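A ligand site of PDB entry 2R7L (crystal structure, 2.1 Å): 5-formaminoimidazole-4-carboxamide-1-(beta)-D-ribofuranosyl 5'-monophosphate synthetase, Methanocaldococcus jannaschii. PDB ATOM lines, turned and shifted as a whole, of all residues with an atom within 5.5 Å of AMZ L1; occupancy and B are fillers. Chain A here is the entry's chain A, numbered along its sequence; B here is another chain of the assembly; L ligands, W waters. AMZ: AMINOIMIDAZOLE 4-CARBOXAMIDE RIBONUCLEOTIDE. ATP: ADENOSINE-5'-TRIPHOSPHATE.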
ATOM      1  N   SER A  26      18.748  -8.364 -20.903  1.00  0.00           N
ATOM      2  CA  SER A  26      20.112  -7.867 -20.897  1.00  0.00           C
ATOM      3  C   SER A  26      20.316  -6.959 -19.706  1.00  0.00           C
ATOM      4  O   SER A  26      19.375  -6.685 -18.957  1.00  0.00           O
ATOM      5  CB  SER A  26      20.406  -7.077 -22.178  1.00  0.00           C
ATOM      6  OG  SER A  26      21.777  -6.740 -22.253  1.00  0.00           O
ATOM      7  N   HIS A  27      21.550  -6.461 -19.547  1.00  0.00           N
ATOM      8  CA  HIS A  27      21.884  -5.442 -18.558  1.00  0.00           C
ATOM      9  C   HIS A  27      21.785  -5.924 -17.108  1.00  0.00           C
ATOM     10  O   HIS A  27      22.796  -6.222 -16.486  1.00  0.00           O
ATOM     11  CB  HIS A  27      21.032  -4.187 -18.743  1.00  0.00           C
ATOM     12  CG  HIS A  27      21.527  -3.007 -17.988  1.00  0.00           C
ATOM     13  ND1 HIS A  27      20.966  -2.584 -16.809  1.00  0.00           N
ATOM     14  CD2 HIS A  27      22.557  -2.158 -18.242  1.00  0.00           C
ATOM     15  CE1 HIS A  27      21.610  -1.517 -16.367  1.00  0.00           C
ATOM     16  NE2 HIS A  27      22.582  -1.242 -17.217  1.00  0.00           N
ATOM     17  N   ARG A  51      20.909 -14.823 -28.186  1.00  0.00           N
ATOM     18  CA  ARG A  51      21.048 -14.147 -26.886  1.00  0.00           C
ATOM     19  C   ARG A  51      20.039 -14.595 -25.816  1.00  0.00           C
ATOM     20  O   ARG A  51      19.838 -13.900 -24.809  1.00  0.00           O
ATOM     21  CB  ARG A  51      20.965 -12.632 -27.068  1.00  0.00           C
ATOM     22  CG  ARG A  51      22.086 -12.056 -27.945  1.00  0.00           C
ATOM     23  CD  ARG A  51      22.055 -10.536 -27.947  1.00  0.00           C
ATOM     24  NE  ARG A  51      22.391  -9.964 -26.649  1.00  0.00           N
ATOM     25  CZ  ARG A  51      22.590  -8.663 -26.425  1.00  0.00           C
ATOM     26  NH1 ARG A  51      22.488  -7.796 -27.436  1.00  0.00           N
ATOM     27  NH2 ARG A  51      22.889  -8.221 -25.211  1.00  0.00           N
ATOM     28  N   GLY A  93      19.484   0.164 -18.616  1.00  0.00           N
ATOM     29  CA  GLY A  93      20.458   0.662 -19.588  1.00  0.00           C
ATOM     30  C   GLY A  93      20.282   0.185 -21.017  1.00  0.00           C
ATOM     31  O   GLY A  93      20.133   0.993 -21.931  1.00  0.00           O
ATOM     32  N   SER A  94      20.324  -1.139 -21.204  1.00  0.00           N
ATOM     33  CA  SER A  94      20.230  -1.727 -22.536  1.00  0.00           C
ATOM     34  C   SER A  94      18.882  -1.470 -23.188  1.00  0.00           C
ATOM     35  O   SER A  94      18.786  -1.391 -24.406  1.00  0.00           O
ATOM     36  CB  SER A  94      20.471  -3.229 -22.485  1.00  0.00           C
ATOM     37  OG  SER A  94      21.782  -3.534 -22.090  1.00  0.00           O
ATOM     38  N   TYR A  98      18.501   0.369 -26.739  1.00  0.00           N
ATOM     39  CA  TYR A  98      17.991  -0.367 -27.890  1.00  0.00           C
ATOM     40  C   TYR A  98      16.641   0.161 -28.362  1.00  0.00           C
ATOM     41  O   TYR A  98      16.321   0.115 -29.549  1.00  0.00           O
ATOM     42  CB  TYR A  98      17.870  -1.856 -27.577  1.00  0.00           C
ATOM     43  CG  TYR A  98      19.124  -2.661 -27.764  1.00  0.00           C
ATOM     44  CD1 TYR A  98      19.746  -3.279 -26.683  1.00  0.00           C
ATOM     45  CD2 TYR A  98      19.688  -2.831 -29.025  1.00  0.00           C
ATOM     46  CE1 TYR A  98      20.892  -4.039 -26.859  1.00  0.00           C
ATOM     47  CE2 TYR A  98      20.834  -3.591 -29.202  1.00  0.00           C
ATOM     48  CZ  TYR A  98      21.432  -4.186 -28.115  1.00  0.00           C
ATOM     49  OH  TYR A  98      22.572  -4.944 -28.275  1.00  0.00           O
ATOM     50  N   ASP A 226      29.066  -1.773  -5.446  1.00  0.00           N
ATOM     51  CA  ASP A 226      30.093  -2.495  -6.198  1.00  0.00           C
ATOM     52  C   ASP A 226      31.212  -1.550  -6.599  1.00  0.00           C
ATOM     53  O   ASP A 226      31.064  -0.325  -6.556  1.00  0.00           O
ATOM     54  CB  ASP A 226      29.495  -3.141  -7.458  1.00  0.00           C
ATOM     55  CG  ASP A 226      29.111  -2.111  -8.525  1.00  0.00           C
ATOM     56  OD1 ASP A 226      28.110  -1.400  -8.311  1.00  0.00           O
ATOM     57  OD2 ASP A 226      29.806  -2.018  -9.567  1.00  0.00           O
ATOM     58  N   ARG A 228      33.750  -1.048 -10.029  1.00  0.00           N
ATOM     59  CA  ARG A 228      33.801  -1.446 -11.430  1.00  0.00           C
ATOM     60  C   ARG A 228      35.019  -2.291 -11.721  1.00  0.00           C
ATOM     61  O   ARG A 228      36.054  -2.142 -11.075  1.00  0.00           O
ATOM     62  CB  ARG A 228      33.827  -0.212 -12.341  1.00  0.00           C
ATOM     63  CG  ARG A 228      32.686   0.749 -12.142  1.00  0.00           C
ATOM     64  CD  ARG A 228      31.355   0.060 -12.352  1.00  0.00           C
ATOM     65  NE  ARG A 228      30.357   0.975 -12.890  1.00  0.00           N
ATOM     66  CZ  ARG A 228      29.057   0.899 -12.621  1.00  0.00           C
ATOM     67  NH1 ARG A 228      28.588  -0.050 -11.828  1.00  0.00           N
ATOM     68  NH2 ARG A 228      28.214   1.783 -13.158  1.00  0.00           N
ATOM     69  N   ILE A 255      33.434  -1.100 -19.325  1.00  0.00           N
ATOM     70  CA  ILE A 255      32.865  -1.901 -18.229  1.00  0.00           C
ATOM     71  C   ILE A 255      32.777  -3.368 -18.615  1.00  0.00           C
ATOM     72  O   ILE A 255      32.174  -3.720 -19.643  1.00  0.00           O
ATOM     73  CB  ILE A 255      31.465  -1.396 -17.762  1.00  0.00           C
ATOM     74  CG1 ILE A 255      31.086  -2.067 -16.434  1.00  0.00           C
ATOM     75  CG2 ILE A 255      30.382  -1.666 -18.809  1.00  0.00           C
ATOM     76  CD1 ILE A 255      32.042  -1.746 -15.296  1.00  0.00           C
ATOM     77  N   GLY A 257      32.562  -5.881 -15.773  1.00  0.00           N
ATOM     78  CA  GLY A 257      32.083  -6.637 -14.614  1.00  0.00           C
ATOM     79  C   GLY A 257      32.163  -5.836 -13.339  1.00  0.00           C
ATOM     80  O   GLY A 257      32.546  -4.666 -13.347  1.00  0.00           O
ATOM     81  N   ASN A 258      31.794  -6.481 -12.233  1.00  0.00           N
ATOM     82  CA  ASN A 258      31.698  -5.798 -10.951  1.00  0.00           C
ATOM     83  C   ASN A 258      32.189  -6.678  -9.811  1.00  0.00           C
ATOM     84  O   ASN A 258      32.108  -7.892  -9.852  1.00  0.00           O
ATOM     85  CB  ASN A 258      30.250  -5.360 -10.678  1.00  0.00           C
ATOM     86  CG  ASN A 258      29.597  -4.687 -11.894  1.00  0.00           C
ATOM     87  OD1 ASN A 258      29.470  -3.463 -11.944  1.00  0.00           O
ATOM     88  ND2 ASN A 258      29.187  -5.493 -12.859  1.00  0.00           N
ATOM     89  N   ARG A 314      17.782   5.105 -13.087  1.00  0.00           N
ATOM     90  CA  ARG A 314      17.143   3.799 -12.997  1.00  0.00           C
ATOM     91  C   ARG A 314      18.179   2.789 -12.498  1.00  0.00           C
ATOM     92  O   ARG A 314      19.195   3.169 -11.926  1.00  0.00           O
ATOM     93  CB  ARG A 314      16.539   3.401 -14.335  1.00  0.00           C
ATOM     94  CG  ARG A 314      17.324   3.874 -15.542  1.00  0.00           C
ATOM     95  CD  ARG A 314      18.624   3.136 -15.650  1.00  0.00           C
ATOM     96  NE  ARG A 314      19.469   3.708 -16.675  1.00  0.00           N
ATOM     97  CZ  ARG A 314      20.635   3.202 -17.058  1.00  0.00           C
ATOM     98  NH1 ARG A 314      21.341   3.799 -18.001  1.00  0.00           N
ATOM     99  NH2 ARG A 314      21.083   2.087 -16.483  1.00  0.00           N
ATOM    100  N   ASP A 316      21.233   0.481 -12.064  1.00  0.00           N
ATOM    101  CA  ASP A 316      22.605   0.419 -12.573  1.00  0.00           C
ATOM    102  C   ASP A 316      23.100  -1.029 -12.688  1.00  0.00           C
ATOM    103  O   ASP A 316      22.747  -1.883 -11.873  1.00  0.00           O
ATOM    104  CB  ASP A 316      23.538   1.233 -11.678  1.00  0.00           C
ATOM    105  CG  ASP A 316      25.002   1.140 -12.104  1.00  0.00           C
ATOM    106  OD1 ASP A 316      25.460   2.056 -12.827  1.00  0.00           O
ATOM    107  OD2 ASP A 316      25.683   0.161 -11.749  1.00  0.00           O
ATOM    108  N   GLY A 317      23.933  -1.290 -13.687  1.00  0.00           N
ATOM    109  CA  GLY A 317      24.426  -2.641 -13.957  1.00  0.00           C
ATOM    110  C   GLY A 317      25.139  -3.313 -12.798  1.00  0.00           C
ATOM    111  O   GLY A 317      25.198  -4.537 -12.733  1.00  0.00           O
ATOM    112  N   GLY A 318      25.679  -2.514 -11.884  1.00  0.00           N
ATOM    113  CA  GLY A 318      26.435  -3.052 -10.758  1.00  0.00           C
ATOM    114  C   GLY A 318      25.630  -3.809  -9.719  1.00  0.00           C
ATOM    115  O   GLY A 318      26.200  -4.471  -8.838  1.00  0.00           O
ATOM    116  N   ASN A 320      24.135  -6.305 -10.289  1.00  0.00           N
ATOM    117  CA  ASN A 320      24.395  -7.696 -10.576  1.00  0.00           C
ATOM    118  C   ASN A 320      25.349  -8.347  -9.571  1.00  0.00           C
ATOM    119  O   ASN A 320      25.329  -9.557  -9.390  1.00  0.00           O
ATOM    120  CB  ASN A 320      24.905  -7.871 -12.018  1.00  0.00           C
ATOM    121  CG  ASN A 320      23.857  -7.465 -13.052  1.00  0.00           C
ATOM    122  OD1 ASN A 320      22.654  -7.552 -12.804  1.00  0.00           O
ATOM    123  ND2 ASN A 320      24.324  -7.033 -14.217  1.00  0.00           N
ATOM    124  N   ILE B 263      30.106 -10.780 -14.387  1.00  0.00           N
ATOM    125  CA  ILE B 263      30.409 -10.233 -15.683  1.00  0.00           C
ATOM    126  C   ILE B 263      29.265  -9.335 -16.155  1.00  0.00           C
ATOM    127  O   ILE B 263      28.134  -9.453 -15.675  1.00  0.00           O
ATOM    128  CB  ILE B 263      30.654 -11.346 -16.722  1.00  0.00           C
ATOM    129  CG1 ILE B 263      31.561 -10.856 -17.855  1.00  0.00           C
ATOM    130  CG2 ILE B 263      29.320 -11.878 -17.261  1.00  0.00           C
ATOM    131  CD1 ILE B 263      32.093 -11.985 -18.743  1.00  0.00           C
ATOM    132  N   ARG B 264      29.568  -8.442 -17.086  1.00  0.00           N
ATOM    133  CA  ARG B 264      28.570  -7.618 -17.769  1.00  0.00           C
ATOM    134  C   ARG B 264      27.549  -8.564 -18.396  1.00  0.00           C
ATOM    135  O   ARG B 264      27.928  -9.505 -19.106  1.00  0.00           O
ATOM    136  CB  ARG B 264      29.273  -6.795 -18.842  1.00  0.00           C
ATOM    137  CG  ARG B 264      28.407  -5.867 -19.649  1.00  0.00           C
ATOM    138  CD  ARG B 264      29.345  -4.967 -20.456  1.00  0.00           C
ATOM    139  NE  ARG B 264      28.662  -4.125 -21.438  1.00  0.00           N
ATOM    140  CZ  ARG B 264      29.254  -3.143 -22.108  1.00  0.00           C
ATOM    141  NH1 ARG B 264      30.526  -2.860 -21.894  1.00  0.00           N
ATOM    142  NH2 ARG B 264      28.571  -2.435 -22.987  1.00  0.00           N
ATOM    143  N   GLU B 265      26.260  -8.330 -18.145  1.00  0.00           N
ATOM    144  CA  GLU B 265      25.238  -9.327 -18.480  1.00  0.00           C
ATOM    145  C   GLU B 265      25.153  -9.612 -19.981  1.00  0.00           C
ATOM    146  O   GLU B 265      24.969 -10.755 -20.381  1.00  0.00           O
ATOM    147  CB  GLU B 265      23.858  -8.933 -17.917  1.00  0.00           C
ATOM    148  CG  GLU B 265      22.836 -10.078 -17.920  1.00  0.00           C
ATOM    149  CD  GLU B 265      21.508  -9.694 -17.283  1.00  0.00           C
ATOM    150  OE1 GLU B 265      21.468  -9.487 -16.051  1.00  0.00           O
ATOM    151  OE2 GLU B 265      20.499  -9.599 -18.025  1.00  0.00           O
ATOM    152  N   SER B 266      25.306  -8.578 -20.814  1.00  0.00           N
ATOM    153  CA  SER B 266      25.319  -8.762 -22.269  1.00  0.00           C
ATOM    154  C   SER B 266      26.379  -9.748 -22.765  1.00  0.00           C
ATOM    155  O   SER B 266      26.360 -10.159 -23.920  1.00  0.00           O
ATOM    156  CB  SER B 266      25.485  -7.410 -22.992  1.00  0.00           C
ATOM    157  OG  SER B 266      26.595  -6.681 -22.478  1.00  0.00           O
HETATM  158  O5  AMZ L   1      28.011  -4.212 -15.063  1.00  0.00           O
HETATM  159  C6  AMZ L   1      27.901  -2.994 -15.192  1.00  0.00           C
HETATM  160  N2  AMZ L   1      28.324  -2.095 -14.299  1.00  0.00           N
HETATM  161  C3A AMZ L   1      27.255  -2.398 -16.438  1.00  0.00           C
HETATM  162  C7A AMZ L   1      27.167  -1.062 -16.779  1.00  0.00           C
HETATM  163  N3  AMZ L   1      27.624  -0.011 -16.085  1.00  0.00           N
HETATM  164  N1  AMZ L   1      26.700  -3.110 -17.410  1.00  0.00           N
HETATM  165  C5  AMZ L   1      26.266  -2.241 -18.328  1.00  0.00           C
HETATM  166  N   AMZ L   1      26.555  -0.992 -17.944  1.00  0.00           N
HETATM  167  C1  AMZ L   1      26.232   0.251 -18.682  1.00  0.00           C
HETATM  168  C2  AMZ L   1      27.314   0.644 -19.687  1.00  0.00           C
HETATM  169  C3  AMZ L   1      26.749   0.181 -21.023  1.00  0.00           C
HETATM  170  O2  AMZ L   1      27.124   1.101 -22.035  1.00  0.00           O
HETATM  171  O1  AMZ L   1      27.417   2.074 -19.676  1.00  0.00           O
HETATM  172  O   AMZ L   1      25.047  -0.080 -19.428  1.00  0.00           O
HETATM  173  C   AMZ L   1      25.246   0.286 -20.805  1.00  0.00           C
HETATM  174  C4  AMZ L   1      24.462  -0.743 -21.649  1.00  0.00           C
HETATM  175  O3  AMZ L   1      24.923  -2.058 -21.361  1.00  0.00           O
HETATM  176  P   AMZ L   1      25.142  -3.089 -22.544  1.00  0.00           P
HETATM  177  OP1 AMZ L   1      23.910  -3.478 -23.276  1.00  0.00           O
HETATM  178  O4  AMZ L   1      26.192  -2.415 -23.561  1.00  0.00           O
HETATM  179  OP2 AMZ L   1      25.887  -4.380 -21.923  1.00  0.00           O
HETATM  180  PG  ATP L   2      29.769   2.918 -17.211  1.00  0.00           P
HETATM  181  O1G ATP L   2      28.288   2.818 -17.541  1.00  0.00           O
HETATM  182  O2G ATP L   2      30.066   2.996 -15.727  1.00  0.00           O
HETATM  183  O3G ATP L   2      30.626   1.933 -17.964  1.00  0.00           O
HETATM  184  PB  ATP L   2      29.777   5.771 -17.138  1.00  0.00           P
HETATM  185  O1B ATP L   2      28.743   5.518 -16.064  1.00  0.00           O
HETATM  186  O2B ATP L   2      29.448   6.737 -18.248  1.00  0.00           O
HETATM  187  O3B ATP L   2      30.199   4.359 -17.809  1.00  0.00           O
HETATM  188  PA  ATP L   2      32.309   7.131 -17.032  1.00  0.00           P
HETATM  189  O1A ATP L   2      32.146   8.572 -16.604  1.00  0.00           O
HETATM  190  O2A ATP L   2      32.472   6.746 -18.469  1.00  0.00           O
HETATM  191  O3A ATP L   2      31.098   6.272 -16.366  1.00  0.00           O
HETATM  192  O5' ATP L   2      33.574   6.567 -16.218  1.00  0.00           O
HETATM  193  C5' ATP L   2      34.200   5.379 -16.671  1.00  0.00           C
HETATM  194  C4' ATP L   2      35.340   5.075 -15.715  1.00  0.00           C
HETATM  195  O4' ATP L   2      36.353   6.080 -15.803  1.00  0.00           O
HETATM  196  C3' ATP L   2      34.902   5.076 -14.254  1.00  0.00           C
HETATM  197  O3' ATP L   2      34.399   3.800 -13.851  1.00  0.00           O
HETATM  198  C2' ATP L   2      36.178   5.450 -13.526  1.00  0.00           C
HETATM  199  O2' ATP L   2      36.972   4.289 -13.291  1.00  0.00           O
HETATM  200  C1' ATP L   2      36.915   6.343 -14.513  1.00  0.00           C
HETATM  201  N9  ATP L   2      36.612   7.750 -14.164  1.00  0.00           N
HETATM  202  C8  ATP L   2      35.536   8.430 -14.599  1.00  0.00           C
HETATM  203  N7  ATP L   2      35.525   9.692 -14.091  1.00  0.00           N
HETATM  204  C5  ATP L   2      36.623   9.828 -13.321  1.00  0.00           C
HETATM  205  C6  ATP L   2      37.214  10.908 -12.510  1.00  0.00           C
HETATM  206  N6  ATP L   2      36.619  12.114 -12.408  1.00  0.00           N
HETATM  207  N1  ATP L   2      38.364  10.629 -11.858  1.00  0.00           N
HETATM  208  C2  ATP L   2      38.960   9.415 -11.940  1.00  0.00           C
HETATM  209  N3  ATP L   2      38.481   8.395 -12.674  1.00  0.00           N
HETATM  210  C4  ATP L   2      37.323   8.534 -13.359  1.00  0.00           C
HETATM  211  O   HOH W   1      27.322  -4.045 -25.373  1.00  0.00           O
HETATM  212  O   HOH W   2      24.849  -6.182 -19.964  1.00  0.00           O
HETATM  213  O   HOH W   3      23.574   2.940 -18.871  1.00  0.00           O
HETATM  214  O   HOH W   4      27.533  -7.371 -14.281  1.00  0.00           O
HETATM  215  O   HOH W   5      25.433  -5.868 -17.425  1.00  0.00           O
HETATM  216  O   HOH W   6      23.333  -1.355 -25.459  1.00  0.00           O
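The side-chain hydroxyl of Ser 94 sits at hydrogen-bond distance from an oxygen (OP1) of AMZ L1 (2.4 Å).
The guanidinium group (NH2) of Arg 264 of chain B is in salt-bridge range of an oxygen (O4) of AMZ L1 (2.4 Å).
An oxygen (OP2) of AMZ L1 sits at hydrogen-bond distance from the side-chain hydroxyl of Ser 266 of chain B.
O5 of AMZ L1 is in hydrogen-bond range of ND2 of Asn 258.
An oxygen (O2G) of ATP L2 is in salt-bridge range of the guanidinium group (NH2) of Arg 228, at 3.4 Å.
O1 of AMZ L1 is in hydrogen-bond range of O1G of ATP L2 (2.4 Å).
The side-chain hydroxyl of Ser 94 lies within hydrogen-bond range of the side-chain hydroxyl of Ser 26 (3.2 Å).
The guanidinium group (NE) of Arg 264 of chain B lies within hydrogen-bond range of the side-chain hydroxyl (OG) of Ser 266 of chain B (3.4 Å).
NH1 of Arg 264 of chain B is in hydrogen-bond range of O of Ile 255 (2.9 Å).
OD1 of Asn 258 lies close to OD2 of Asp 226, 2.8 Å away.
NH2 of Arg 228 lies within salt-bridge range of OD1 of Asp 316, 2.8 Å away.
The guanidinium group (NH1) of Arg 228 is in salt-bridge range of the side-chain carboxylate (OD2) of Asp 226, 3.2 Å away.
The side-chain carboxylate of Asp 316 lies within hydrogen-bond range of the backbone NH of Gly 318 (2.7 Å).
The backbone carbonyl oxygen (O) of Gly 317 lies within hydrogen-bond range of the side-chain amide nitrogen (ND2) of Asn 320.
N2 of AMZ L1 sits close to NH1 of Arg 228.
His 27 touches AMZ L1 (CD2 to O, 3.5 Å).
Ile 255 touches AMZ L1.
O of Gly 317 touches O5 of AMZ L1 (3.7 Å).
Gly 318 touches AMZ L1.
Hydrophobic or aromatic side chains within 4 Å of AMZ L1: His 27 and Ile 255.
Nine residues have an atom within 4 Å of AMZ L1: His 27, Ser 94, Arg 228, Ile 255, Asn 258, Gly 317, Gly 318, Arg 264 of chain B and Ser 266 of chain B.
The nearest printed residue that does not touch AMZ L1 is Ser 26 (4.03 Å).
Water W1 bridges an oxygen (O4) of AMZ L1 (2.7 Å) and the guanidinium group of Arg 264 of chain B (3.1 Å).
Water W5 lies within hydrogen-bond range of the backbone NH of Glu 265 of chain B, the backbone carbonyl oxygen of His 27 and a nitrogen (N1) of AMZ L1.
Water W4 lies within hydrogen-bond range of O of Ile 263 of chain B (2.6 Å), ND2 of Asn 258 (2.9 Å), ND2 of Asn 320 (3.2 Å) and O5 of AMZ L1 (3.3 Å).
Water W3 bridges the guanidinium group (NH1) of Arg 314 (2.5 Å) and an oxygen (O) of AMZ L1 (3.4 Å).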
